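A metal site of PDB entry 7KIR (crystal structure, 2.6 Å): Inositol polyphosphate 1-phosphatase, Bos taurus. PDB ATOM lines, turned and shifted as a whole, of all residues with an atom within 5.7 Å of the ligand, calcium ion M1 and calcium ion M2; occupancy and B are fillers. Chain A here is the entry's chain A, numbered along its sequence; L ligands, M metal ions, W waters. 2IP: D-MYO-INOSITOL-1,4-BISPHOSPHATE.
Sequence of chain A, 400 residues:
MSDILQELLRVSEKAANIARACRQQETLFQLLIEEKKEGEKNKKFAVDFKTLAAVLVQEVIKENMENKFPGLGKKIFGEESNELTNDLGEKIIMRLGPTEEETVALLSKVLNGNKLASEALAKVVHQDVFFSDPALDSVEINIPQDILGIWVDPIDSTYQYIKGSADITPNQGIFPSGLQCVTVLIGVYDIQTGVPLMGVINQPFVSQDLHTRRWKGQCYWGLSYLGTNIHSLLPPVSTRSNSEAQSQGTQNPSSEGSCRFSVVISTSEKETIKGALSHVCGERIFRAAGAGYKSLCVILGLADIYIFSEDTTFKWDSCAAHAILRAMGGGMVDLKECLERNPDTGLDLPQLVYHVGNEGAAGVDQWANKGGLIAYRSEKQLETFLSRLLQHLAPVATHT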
ATOM      1  N   LYS A  50     -22.312 -24.558  22.496  1.00  0.00           N
ATOM      2  CA  LYS A  50     -21.559 -24.141  21.323  1.00  0.00           C
ATOM      3  C   LYS A  50     -21.836 -25.062  20.138  1.00  0.00           C
ATOM      4  O   LYS A  50     -22.119 -24.596  19.019  1.00  0.00           O
ATOM      5  CB  LYS A  50     -20.060 -24.047  21.645  1.00  0.00           C
ATOM      6  CG  LYS A  50     -19.333 -25.381  21.905  1.00  0.00           C
ATOM      7  CD  LYS A  50     -17.983 -25.443  21.203  1.00  0.00           C
ATOM      8  CE  LYS A  50     -17.502 -26.862  20.978  1.00  0.00           C
ATOM      9  NZ  LYS A  50     -16.616 -26.932  19.779  1.00  0.00           N
ATOM     10  N   GLU A  79     -18.501 -29.153   8.953  1.00  0.00           N
ATOM     11  CA  GLU A  79     -17.776 -29.651  10.117  1.00  0.00           C
ATOM     12  C   GLU A  79     -18.700 -30.342  11.116  1.00  0.00           C
ATOM     13  O   GLU A  79     -18.269 -31.264  11.818  1.00  0.00           O
ATOM     14  CB  GLU A  79     -17.028 -28.503  10.795  1.00  0.00           C
ATOM     15  CG  GLU A  79     -16.180 -28.937  11.967  1.00  0.00           C
ATOM     16  CD  GLU A  79     -15.588 -27.768  12.696  1.00  0.00           C
ATOM     17  OE1 GLU A  79     -16.004 -26.628  12.400  1.00  0.00           O
ATOM     18  OE2 GLU A  79     -14.706 -27.983  13.559  1.00  0.00           O
ATOM     19  N   GLU A  80     -19.954 -29.931  11.193  1.00  0.00           N
ATOM     20  CA  GLU A  80     -20.844 -30.434  12.225  1.00  0.00           C
ATOM     21  C   GLU A  80     -21.706 -31.574  11.698  1.00  0.00           C
ATOM     22  O   GLU A  80     -22.050 -31.646  10.514  1.00  0.00           O
ATOM     23  CB  GLU A  80     -21.730 -29.316  12.771  1.00  0.00           C
ATOM     24  CG  GLU A  80     -20.946 -28.213  13.453  1.00  0.00           C
ATOM     25  CD  GLU A  80     -20.003 -28.746  14.513  1.00  0.00           C
ATOM     26  OE1 GLU A  80     -20.405 -29.652  15.272  1.00  0.00           O
ATOM     27  OE2 GLU A  80     -18.860 -28.266  14.589  1.00  0.00           O
ATOM     28  N   ASP A 153     -18.135 -24.229   7.251  1.00  0.00           N
ATOM     29  CA  ASP A 153     -17.863 -24.087   8.669  1.00  0.00           C
ATOM     30  C   ASP A 153     -18.870 -23.100   9.233  1.00  0.00           C
ATOM     31  O   ASP A 153     -18.770 -21.894   8.944  1.00  0.00           O
ATOM     32  CB  ASP A 153     -16.436 -23.605   8.918  1.00  0.00           C
ATOM     33  CG  ASP A 153     -16.034 -23.771  10.365  1.00  0.00           C
ATOM     34  OD1 ASP A 153     -16.919 -24.008  11.198  1.00  0.00           O
ATOM     35  OD2 ASP A 153     -14.825 -23.670  10.669  1.00  0.00           O
ATOM     36  N   PRO A 154     -19.847 -23.562  10.005  1.00  0.00           N
ATOM     37  CA  PRO A 154     -20.880 -22.644  10.515  1.00  0.00           C
ATOM     38  C   PRO A 154     -20.318 -21.547  11.416  1.00  0.00           C
ATOM     39  O   PRO A 154     -20.737 -20.391  11.296  1.00  0.00           O
ATOM     40  CB  PRO A 154     -21.837 -23.577  11.256  1.00  0.00           C
ATOM     41  CG  PRO A 154     -21.029 -24.822  11.529  1.00  0.00           C
ATOM     42  CD  PRO A 154     -20.097 -24.955  10.391  1.00  0.00           C
ATOM     43  N   ILE A 155     -19.400 -21.876  12.323  1.00  0.00           N
ATOM     44  CA  ILE A 155     -18.771 -20.885  13.190  1.00  0.00           C
ATOM     45  C   ILE A 155     -17.296 -21.234  13.322  1.00  0.00           C
ATOM     46  O   ILE A 155     -16.949 -22.231  13.970  1.00  0.00           O
ATOM     47  CB  ILE A 155     -19.416 -20.809  14.588  1.00  0.00           C
ATOM     48  CG1 ILE A 155     -20.910 -20.495  14.527  1.00  0.00           C
ATOM     49  CG2 ILE A 155     -18.665 -19.786  15.450  1.00  0.00           C
ATOM     50  CD1 ILE A 155     -21.635 -20.750  15.835  1.00  0.00           C
ATOM     51  N   ASP A 156     -16.442 -20.421  12.726  1.00  0.00           N
ATOM     52  CA  ASP A 156     -15.003 -20.626  12.842  1.00  0.00           C
ATOM     53  C   ASP A 156     -14.444 -19.764  13.969  1.00  0.00           C
ATOM     54  O   ASP A 156     -14.924 -18.653  14.211  1.00  0.00           O
ATOM     55  CB  ASP A 156     -14.303 -20.299  11.530  1.00  0.00           C
ATOM     56  CG  ASP A 156     -12.836 -20.657  11.557  1.00  0.00           C
ATOM     57  OD1 ASP A 156     -12.533 -21.845  11.766  1.00  0.00           O
ATOM     58  OD2 ASP A 156     -11.974 -19.769  11.381  1.00  0.00           O
ATOM     59  N   SER A 157     -13.425 -20.298  14.649  1.00  0.00           N
ATOM     60  CA  SER A 157     -12.875 -19.751  15.892  1.00  0.00           C
ATOM     61  C   SER A 157     -13.926 -19.777  16.998  1.00  0.00           C
ATOM     62  O   SER A 157     -14.416 -18.758  17.486  1.00  0.00           O
ATOM     63  CB  SER A 157     -12.312 -18.338  15.692  1.00  0.00           C
ATOM     64  OG  SER A 157     -11.508 -17.957  16.789  1.00  0.00           O
ATOM     65  N   THR A 158     -14.273 -21.012  17.394  1.00  0.00           N
ATOM     66  CA  THR A 158     -15.316 -21.215  18.384  1.00  0.00           C
ATOM     67  C   THR A 158     -14.879 -20.714  19.760  1.00  0.00           C
ATOM     68  O   THR A 158     -15.718 -20.227  20.548  1.00  0.00           O
ATOM     69  CB  THR A 158     -15.705 -22.699  18.459  1.00  0.00           C
ATOM     70  OG1 THR A 158     -15.622 -23.271  17.153  1.00  0.00           O
ATOM     71  CG2 THR A 158     -17.119 -22.842  18.950  1.00  0.00           C
ATOM     72  N   TYR A 159     -13.584 -20.796  20.070  1.00  0.00           N
ATOM     73  CA  TYR A 159     -13.100 -20.372  21.374  1.00  0.00           C
ATOM     74  C   TYR A 159     -13.196 -18.850  21.528  1.00  0.00           C
ATOM     75  O   TYR A 159     -13.469 -18.345  22.618  1.00  0.00           O
ATOM     76  CB  TYR A 159     -11.661 -20.849  21.590  1.00  0.00           C
ATOM     77  CG  TYR A 159     -11.067 -20.372  22.888  1.00  0.00           C
ATOM     78  CD1 TYR A 159     -11.377 -20.998  24.095  1.00  0.00           C
ATOM     79  CD2 TYR A 159     -10.190 -19.289  22.922  1.00  0.00           C
ATOM     80  CE1 TYR A 159     -10.838 -20.564  25.280  1.00  0.00           C
ATOM     81  CE2 TYR A 159      -9.645 -18.842  24.107  1.00  0.00           C
ATOM     82  CZ  TYR A 159      -9.975 -19.492  25.286  1.00  0.00           C
ATOM     83  OH  TYR A 159      -9.430 -19.045  26.470  1.00  0.00           O
ATOM     84  N   SER A 268      -1.045 -18.563  13.427  1.00  0.00           N
ATOM     85  CA  SER A 268      -2.090 -18.850  14.400  1.00  0.00           C
ATOM     86  C   SER A 268      -1.537 -18.711  15.821  1.00  0.00           C
ATOM     87  O   SER A 268      -0.361 -18.393  16.035  1.00  0.00           O
ATOM     88  CB  SER A 268      -2.670 -20.235  14.151  1.00  0.00           C
ATOM     89  OG  SER A 268      -2.121 -21.216  15.017  1.00  0.00           O
ATOM     90  N   GLU A 269      -2.391 -18.955  16.812  1.00  0.00           N
ATOM     91  CA  GLU A 269      -2.020 -18.688  18.184  1.00  0.00           C
ATOM     92  C   GLU A 269      -1.136 -19.759  18.797  1.00  0.00           C
ATOM     93  O   GLU A 269      -0.466 -19.503  19.805  1.00  0.00           O
ATOM     94  CB  GLU A 269      -3.284 -18.534  19.026  1.00  0.00           C
ATOM     95  CG  GLU A 269      -4.240 -17.555  18.416  1.00  0.00           C
ATOM     96  CD  GLU A 269      -5.292 -17.109  19.397  1.00  0.00           C
ATOM     97  OE1 GLU A 269      -5.695 -17.925  20.257  1.00  0.00           O
ATOM     98  OE2 GLU A 269      -5.690 -15.922  19.326  1.00  0.00           O
ATOM     99  N   LYS A 270      -1.134 -20.967  18.225  1.00  0.00           N
ATOM    100  CA  LYS A 270      -0.356 -22.065  18.772  1.00  0.00           C
ATOM    101  C   LYS A 270       0.724 -22.523  17.792  1.00  0.00           C
ATOM    102  O   LYS A 270       1.235 -23.641  17.913  1.00  0.00           O
ATOM    103  CB  LYS A 270      -1.269 -23.231  19.145  1.00  0.00           C
ATOM    104  CG  LYS A 270      -2.023 -23.812  17.968  1.00  0.00           C
ATOM    105  CD  LYS A 270      -3.383 -23.166  17.816  1.00  0.00           C
ATOM    106  CE  LYS A 270      -4.398 -24.114  17.196  1.00  0.00           C
ATOM    107  NZ  LYS A 270      -5.743 -23.481  17.258  1.00  0.00           N
ATOM    108  N   ALA A 288      -2.826 -14.285  15.266  1.00  0.00           N
ATOM    109  CA  ALA A 288      -4.265 -14.026  15.168  1.00  0.00           C
ATOM    110  C   ALA A 288      -5.020 -15.338  15.292  1.00  0.00           C
ATOM    111  O   ALA A 288      -4.519 -16.395  14.913  1.00  0.00           O
ATOM    112  CB  ALA A 288      -4.625 -13.328  13.856  1.00  0.00           C
ATOM    113  N   ALA A 289      -6.230 -15.250  15.828  1.00  0.00           N
ATOM    114  CA  ALA A 289      -7.112 -16.401  15.953  1.00  0.00           C
ATOM    115  C   ALA A 289      -8.005 -16.519  14.724  1.00  0.00           C
ATOM    116  O   ALA A 289      -8.341 -15.519  14.085  1.00  0.00           O
ATOM    117  CB  ALA A 289      -7.981 -16.282  17.214  1.00  0.00           C
ATOM    118  N   GLY A 290      -8.355 -17.759  14.391  1.00  0.00           N
ATOM    119  CA  GLY A 290      -9.277 -18.006  13.289  1.00  0.00           C
ATOM    120  C   GLY A 290      -8.615 -18.316  11.961  1.00  0.00           C
ATOM    121  O   GLY A 290      -7.802 -17.536  11.457  1.00  0.00           O
ATOM    122  N   ALA A 291      -8.952 -19.480  11.382  1.00  0.00           N
ATOM    123  CA  ALA A 291      -8.489 -19.800  10.034  1.00  0.00           C
ATOM    124  C   ALA A 291      -9.147 -18.894   9.006  1.00  0.00           C
ATOM    125  O   ALA A 291      -8.480 -18.304   8.146  1.00  0.00           O
ATOM    126  CB  ALA A 291      -8.761 -21.264   9.722  1.00  0.00           C
ATOM    127  N   GLY A 292     -10.478 -18.765   9.102  1.00  0.00           N
ATOM    128  CA  GLY A 292     -11.181 -17.842   8.235  1.00  0.00           C
ATOM    129  C   GLY A 292     -10.687 -16.416   8.386  1.00  0.00           C
ATOM    130  O   GLY A 292     -10.461 -15.730   7.385  1.00  0.00           O
ATOM    131  N   LYS A 294      -7.711 -15.298   9.417  1.00  0.00           N
ATOM    132  CA  LYS A 294      -6.371 -15.080   8.862  1.00  0.00           C
ATOM    133  C   LYS A 294      -6.400 -15.068   7.344  1.00  0.00           C
ATOM    134  O   LYS A 294      -5.764 -14.210   6.710  1.00  0.00           O
ATOM    135  CB  LYS A 294      -5.407 -16.151   9.386  1.00  0.00           C
ATOM    136  CG  LYS A 294      -4.973 -15.907  10.833  1.00  0.00           C
ATOM    137  CD  LYS A 294      -3.899 -16.880  11.305  1.00  0.00           C
ATOM    138  CE  LYS A 294      -4.506 -18.178  11.802  1.00  0.00           C
ATOM    139  NZ  LYS A 294      -5.514 -17.924  12.873  1.00  0.00           N
ATOM    140  N   TYR A 306      -0.164 -16.285   4.844  1.00  0.00           N
ATOM    141  CA  TYR A 306      -0.713 -16.966   6.018  1.00  0.00           C
ATOM    142  C   TYR A 306      -0.184 -18.398   5.979  1.00  0.00           C
ATOM    143  O   TYR A 306      -0.521 -19.168   5.075  1.00  0.00           O
ATOM    144  CB  TYR A 306      -2.241 -16.881   6.011  1.00  0.00           C
ATOM    145  CG  TYR A 306      -3.003 -17.942   6.780  1.00  0.00           C
ATOM    146  CD1 TYR A 306      -2.599 -18.361   8.043  1.00  0.00           C
ATOM    147  CD2 TYR A 306      -4.158 -18.488   6.247  1.00  0.00           C
ATOM    148  CE1 TYR A 306      -3.307 -19.332   8.731  1.00  0.00           C
ATOM    149  CE2 TYR A 306      -4.873 -19.449   6.927  1.00  0.00           C
ATOM    150  CZ  TYR A 306      -4.457 -19.867   8.168  1.00  0.00           C
ATOM    151  OH  TYR A 306      -5.177 -20.818   8.841  1.00  0.00           O
ATOM    152  N   PHE A 308       0.502 -22.137   7.914  1.00  0.00           N
ATOM    153  CA  PHE A 308       0.058 -23.051   8.963  1.00  0.00           C
ATOM    154  C   PHE A 308       0.784 -24.372   8.769  1.00  0.00           C
ATOM    155  O   PHE A 308       0.591 -25.046   7.758  1.00  0.00           O
ATOM    156  CB  PHE A 308      -1.445 -23.247   8.923  1.00  0.00           C
ATOM    157  CG  PHE A 308      -1.999 -23.853  10.170  1.00  0.00           C
ATOM    158  CD1 PHE A 308      -2.270 -25.211  10.235  1.00  0.00           C
ATOM    159  CD2 PHE A 308      -2.219 -23.062  11.288  1.00  0.00           C
ATOM    160  CE1 PHE A 308      -2.776 -25.765  11.396  1.00  0.00           C
ATOM    161  CE2 PHE A 308      -2.710 -23.606  12.450  1.00  0.00           C
ATOM    162  CZ  PHE A 308      -2.996 -24.951  12.506  1.00  0.00           C
ATOM    163  N   THR A 312      -4.023 -29.369  11.438  1.00  0.00           N
ATOM    164  CA  THR A 312      -5.258 -29.185  12.180  1.00  0.00           C
ATOM    165  C   THR A 312      -6.249 -28.248  11.493  1.00  0.00           C
ATOM    166  O   THR A 312      -7.228 -27.832  12.110  1.00  0.00           O
ATOM    167  CB  THR A 312      -4.943 -28.708  13.595  1.00  0.00           C
ATOM    168  OG1 THR A 312      -4.037 -27.596  13.530  1.00  0.00           O
ATOM    169  CG2 THR A 312      -4.286 -29.830  14.388  1.00  0.00           C
ATOM    170  N   THR A 313      -6.034 -27.937  10.215  1.00  0.00           N
ATOM    171  CA  THR A 313      -7.083 -27.311   9.408  1.00  0.00           C
ATOM    172  C   THR A 313      -7.702 -28.361   8.509  1.00  0.00           C
ATOM    173  O   THR A 313      -7.151 -29.455   8.311  1.00  0.00           O
ATOM    174  CB  THR A 313      -6.563 -26.136   8.568  1.00  0.00           C
ATOM    175  OG1 THR A 313      -5.753 -26.630   7.488  1.00  0.00           O
ATOM    176  CG2 THR A 313      -5.770 -25.170   9.413  1.00  0.00           C
ATOM    177  N   PHE A 314      -8.864 -28.022   7.962  1.00  0.00           N
ATOM    178  CA  PHE A 314      -9.651 -28.944   7.143  1.00  0.00           C
ATOM    179  C   PHE A 314     -10.238 -28.175   5.962  1.00  0.00           C
ATOM    180  O   PHE A 314     -10.131 -26.948   5.884  1.00  0.00           O
ATOM    181  CB  PHE A 314     -10.772 -29.612   7.957  1.00  0.00           C
ATOM    182  CG  PHE A 314     -10.319 -30.166   9.278  1.00  0.00           C
ATOM    183  CD1 PHE A 314     -10.013 -31.511   9.411  1.00  0.00           C
ATOM    184  CD2 PHE A 314     -10.201 -29.348  10.392  1.00  0.00           C
ATOM    185  CE1 PHE A 314      -9.594 -32.031  10.623  1.00  0.00           C
ATOM    186  CE2 PHE A 314      -9.775 -29.848  11.610  1.00  0.00           C
ATOM    187  CZ  PHE A 314      -9.477 -31.191  11.729  1.00  0.00           C
ATOM    188  N   TRP A 316     -13.224 -27.353   5.129  1.00  0.00           N
ATOM    189  CA  TRP A 316     -14.183 -26.312   5.443  1.00  0.00           C
ATOM    190  C   TRP A 316     -13.527 -25.059   6.035  1.00  0.00           C
ATOM    191  O   TRP A 316     -14.138 -23.989   5.984  1.00  0.00           O
ATOM    192  CB  TRP A 316     -15.251 -26.836   6.399  1.00  0.00           C
ATOM    193  CG  TRP A 316     -14.708 -27.469   7.636  1.00  0.00           C
ATOM    194  CD1 TRP A 316     -14.309 -26.830   8.783  1.00  0.00           C
ATOM    195  CD2 TRP A 316     -14.517 -28.869   7.868  1.00  0.00           C
ATOM    196  NE1 TRP A 316     -13.868 -27.748   9.713  1.00  0.00           N
ATOM    197  CE2 TRP A 316     -13.985 -29.003   9.175  1.00  0.00           C
ATOM    198  CE3 TRP A 316     -14.731 -30.024   7.101  1.00  0.00           C
ATOM    199  CZ2 TRP A 316     -13.684 -30.253   9.729  1.00  0.00           C
ATOM    200  CZ3 TRP A 316     -14.415 -31.264   7.655  1.00  0.00           C
ATOM    201  CH2 TRP A 316     -13.902 -31.367   8.953  1.00  0.00           C
ATOM    202  N   ASP A 317     -12.326 -25.176   6.592  1.00  0.00           N
ATOM    203  CA  ASP A 317     -11.613 -23.983   7.075  1.00  0.00           C
ATOM    204  C   ASP A 317     -11.132 -23.127   5.925  1.00  0.00           C
ATOM    205  O   ASP A 317     -11.098 -21.892   6.043  1.00  0.00           O
ATOM    206  CB  ASP A 317     -10.418 -24.385   7.938  1.00  0.00           C
ATOM    207  CG  ASP A 317     -10.826 -24.832   9.323  1.00  0.00           C
ATOM    208  OD1 ASP A 317     -11.791 -24.264   9.855  1.00  0.00           O
ATOM    209  OD2 ASP A 317     -10.175 -25.738   9.884  1.00  0.00           O
HETATM  210  C1  2IP L   1     -10.299 -24.136  14.383  1.00  0.00           C
HETATM  211  C2  2IP L   1     -10.251 -22.682  13.980  1.00  0.00           C
HETATM  212  C3  2IP L   1      -9.017 -22.218  14.626  1.00  0.00           C
HETATM  213  C4  2IP L   1      -7.744 -22.823  14.121  1.00  0.00           C
HETATM  214  C5  2IP L   1      -7.857 -24.326  14.349  1.00  0.00           C
HETATM  215  C6  2IP L   1      -9.124 -24.792  13.701  1.00  0.00           C
HETATM  216  O1  2IP L   1     -11.546 -24.591  14.026  1.00  0.00           O
HETATM  217  O2  2IP L   1     -10.040 -22.519  12.617  1.00  0.00           O
HETATM  218  O3  2IP L   1      -9.060 -20.858  14.366  1.00  0.00           O
HETATM  219  O4  2IP L   1      -6.750 -22.464  14.964  1.00  0.00           O
HETATM  220  O5  2IP L   1      -6.693 -24.907  13.846  1.00  0.00           O
HETATM  221  O6  2IP L   1      -9.171 -26.160  13.958  1.00  0.00           O
HETATM  222  P4  2IP L   1      -6.173 -20.931  15.021  1.00  0.00           P
HETATM  223  O41 2IP L   1      -6.024 -20.319  13.667  1.00  0.00           O
HETATM  224  O42 2IP L   1      -4.903 -21.060  15.992  1.00  0.00           O
HETATM  225  O43 2IP L   1      -7.224 -20.061  15.866  1.00  0.00           O
HETATM  226  P1  2IP L   1     -12.762 -24.297  15.046  1.00  0.00           P
HETATM  227  O11 2IP L   1     -13.968 -24.194  14.093  1.00  0.00           O
HETATM  228  O12 2IP L   1     -12.722 -22.983  15.656  1.00  0.00           O
HETATM  229  O13 2IP L   1     -12.923 -25.470  16.089  1.00  0.00           O
HETATM  230 CA    CA M   1     -12.821 -24.203  11.999  1.00  0.00          CA
HETATM  231 CA    CA M   2     -16.188 -24.561  13.535  1.00  0.00          CA
HETATM  232  O   HOH W   1     -15.519 -26.085  15.717  1.00  0.00           O
HETATM  233  O   HOH W   2      -4.782 -21.431  11.495  1.00  0.00           O
HETATM  234  O   HOH W   3     -12.051 -27.071  12.387  1.00  0.00           O
HETATM  235  O   HOH W   4      -9.732 -20.148  16.721  1.00  0.00           O
HETATM  236  O   HOH W   5     -11.646 -22.713  18.030  1.00  0.00           O
HETATM  237  O   HOH W   6     -18.463 -25.505  14.466  1.00  0.00           O
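O11 of the ligand binds calcium ion M2, 2.3 Å away. Calcium ion M2 is bound by OE1 of Glu 79, 2.4 Å away. O of Ile 155 binds calcium ion M2 (2.5 Å). Calcium ion M2 is bound by the side-chain carboxylate (OD1) of Asp 153. Water W6 is bound to calcium ion M2 (2.6 Å). Water W1 is bound to calcium ion M2, 2.7 Å away. Calcium ion M2 has six donor atoms within binding distance.
Calcium ion M1 is bound by OD1 of Asp 317, 2.4 Å away. OD1 of Asp 156 is bound to calcium ion M1 (2.4 Å). Calcium ion M1 is bound by an oxygen (O11) of the ligand, at 2.4 Å. Calcium ion M1 is bound by O1 of the ligand, 2.4 Å away. OD2 of Asp 153 is bound to calcium ion M1 (2.5 Å). Slightly farther from calcium ion M1 lies water W3 (3.0 Å).
Merely in contact with the ligand: Ala 289 (3.7 Å) and Phe 308 (3.9 Å). Of the 26 residues printed, 16 come within 4 Å of the ligand. The nearest printed residue that does not touch the ligand is Ala 288 (4.4 Å).
Water W3 lies within hydrogen-bond range of the side-chain carboxylate (OE2) of Glu 79 (3.0 Å), the indole nitrogen (NE1) of Trp 316 (3.3 Å), the side-chain carboxylate (OD2) of Asp 317 (3.4 Å) and an oxygen (O6) of the ligand (3.4 Å). Water W1 lies within hydrogen-bond range of an oxygen (O13) of the ligand (2.7 Å), the side-chain carboxylate of Glu 79 (3.0 Å) and the side-chain hydroxyl of Thr 158 (3.2 Å). Water W4 bridges O3 of the ligand (2.5 Å) and OG of Ser 157 (2.8 Å). Water W5 lies within hydrogen-bond range of O12 of the ligand (2.6 Å), N of Thr 158 (3.2 Å) and N of Tyr 159 (3.4 Å). Water W2 bridges O41 of the ligand (2.7 Å) and OH of Tyr 306 (2.8 Å).
An oxygen (O12) of the ligand lies within hydrogen-bond range of the backbone NH (N) of Thr 158, 3.1 Å away. O42 of the ligand sits at hydrogen-bond distance from OG of Ser 268 (3.0 Å). N of Gly 290 sits at hydrogen-bond distance from O43 of the ligand. The backbone NH (N) of Ser 157 lies within hydrogen-bond range of an oxygen (O12) of the ligand (3.0 Å). The backbone NH of Ala 291 is in hydrogen-bond range of an oxygen (O3) of the ligand, at 3.3 Å. An oxygen (O12) of the ligand lies within hydrogen-bond range of the side-chain hydroxyl of Thr 158 (3.3 Å). O of Thr 312 sits at hydrogen-bond distance from O6 of the ligand (3.2 Å). O42 of the ligand lies within salt-bridge range of NZ of Lys 270. N of Glu 269 lies within hydrogen-bond range of O42 of the ligand (3.4 Å). The side-chain amino group (NZ) of Lys 294 is in salt-bridge range of an oxygen (O41) of the ligand (2.6 Å).
Residues that only touch calcium ion M2: Thr 158 (3.9 Å). Four residues have an atom within 4 Å of calcium ion M2: Glu 79, Asp 153, Ile 155 and Thr 158. The nearest printed residue that does not touch calcium ion M2 is Asp 156 (4.2 Å).
OD2 of Asp 317 lies within hydrogen-bond range of N of Phe 314 (3.3 Å). The side-chain carboxylate (OD2) of Asp 156 lies within hydrogen-bond range of the backbone NH (N) of Ala 291. NZ of Lys 294 sits at hydrogen-bond distance from O of Ala 288 (2.7 Å). The backbone NH (N) of Lys 270 lies close to the side-chain hydroxyl (OG) of Ser 268 (3.4 Å). The backbone NH of Gly 292 lies within hydrogen-bond range of the side-chain carboxylate of Asp 156, 2.9 Å away. O of Gly 290 lies within hydrogen-bond range of NZ of Lys 294.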
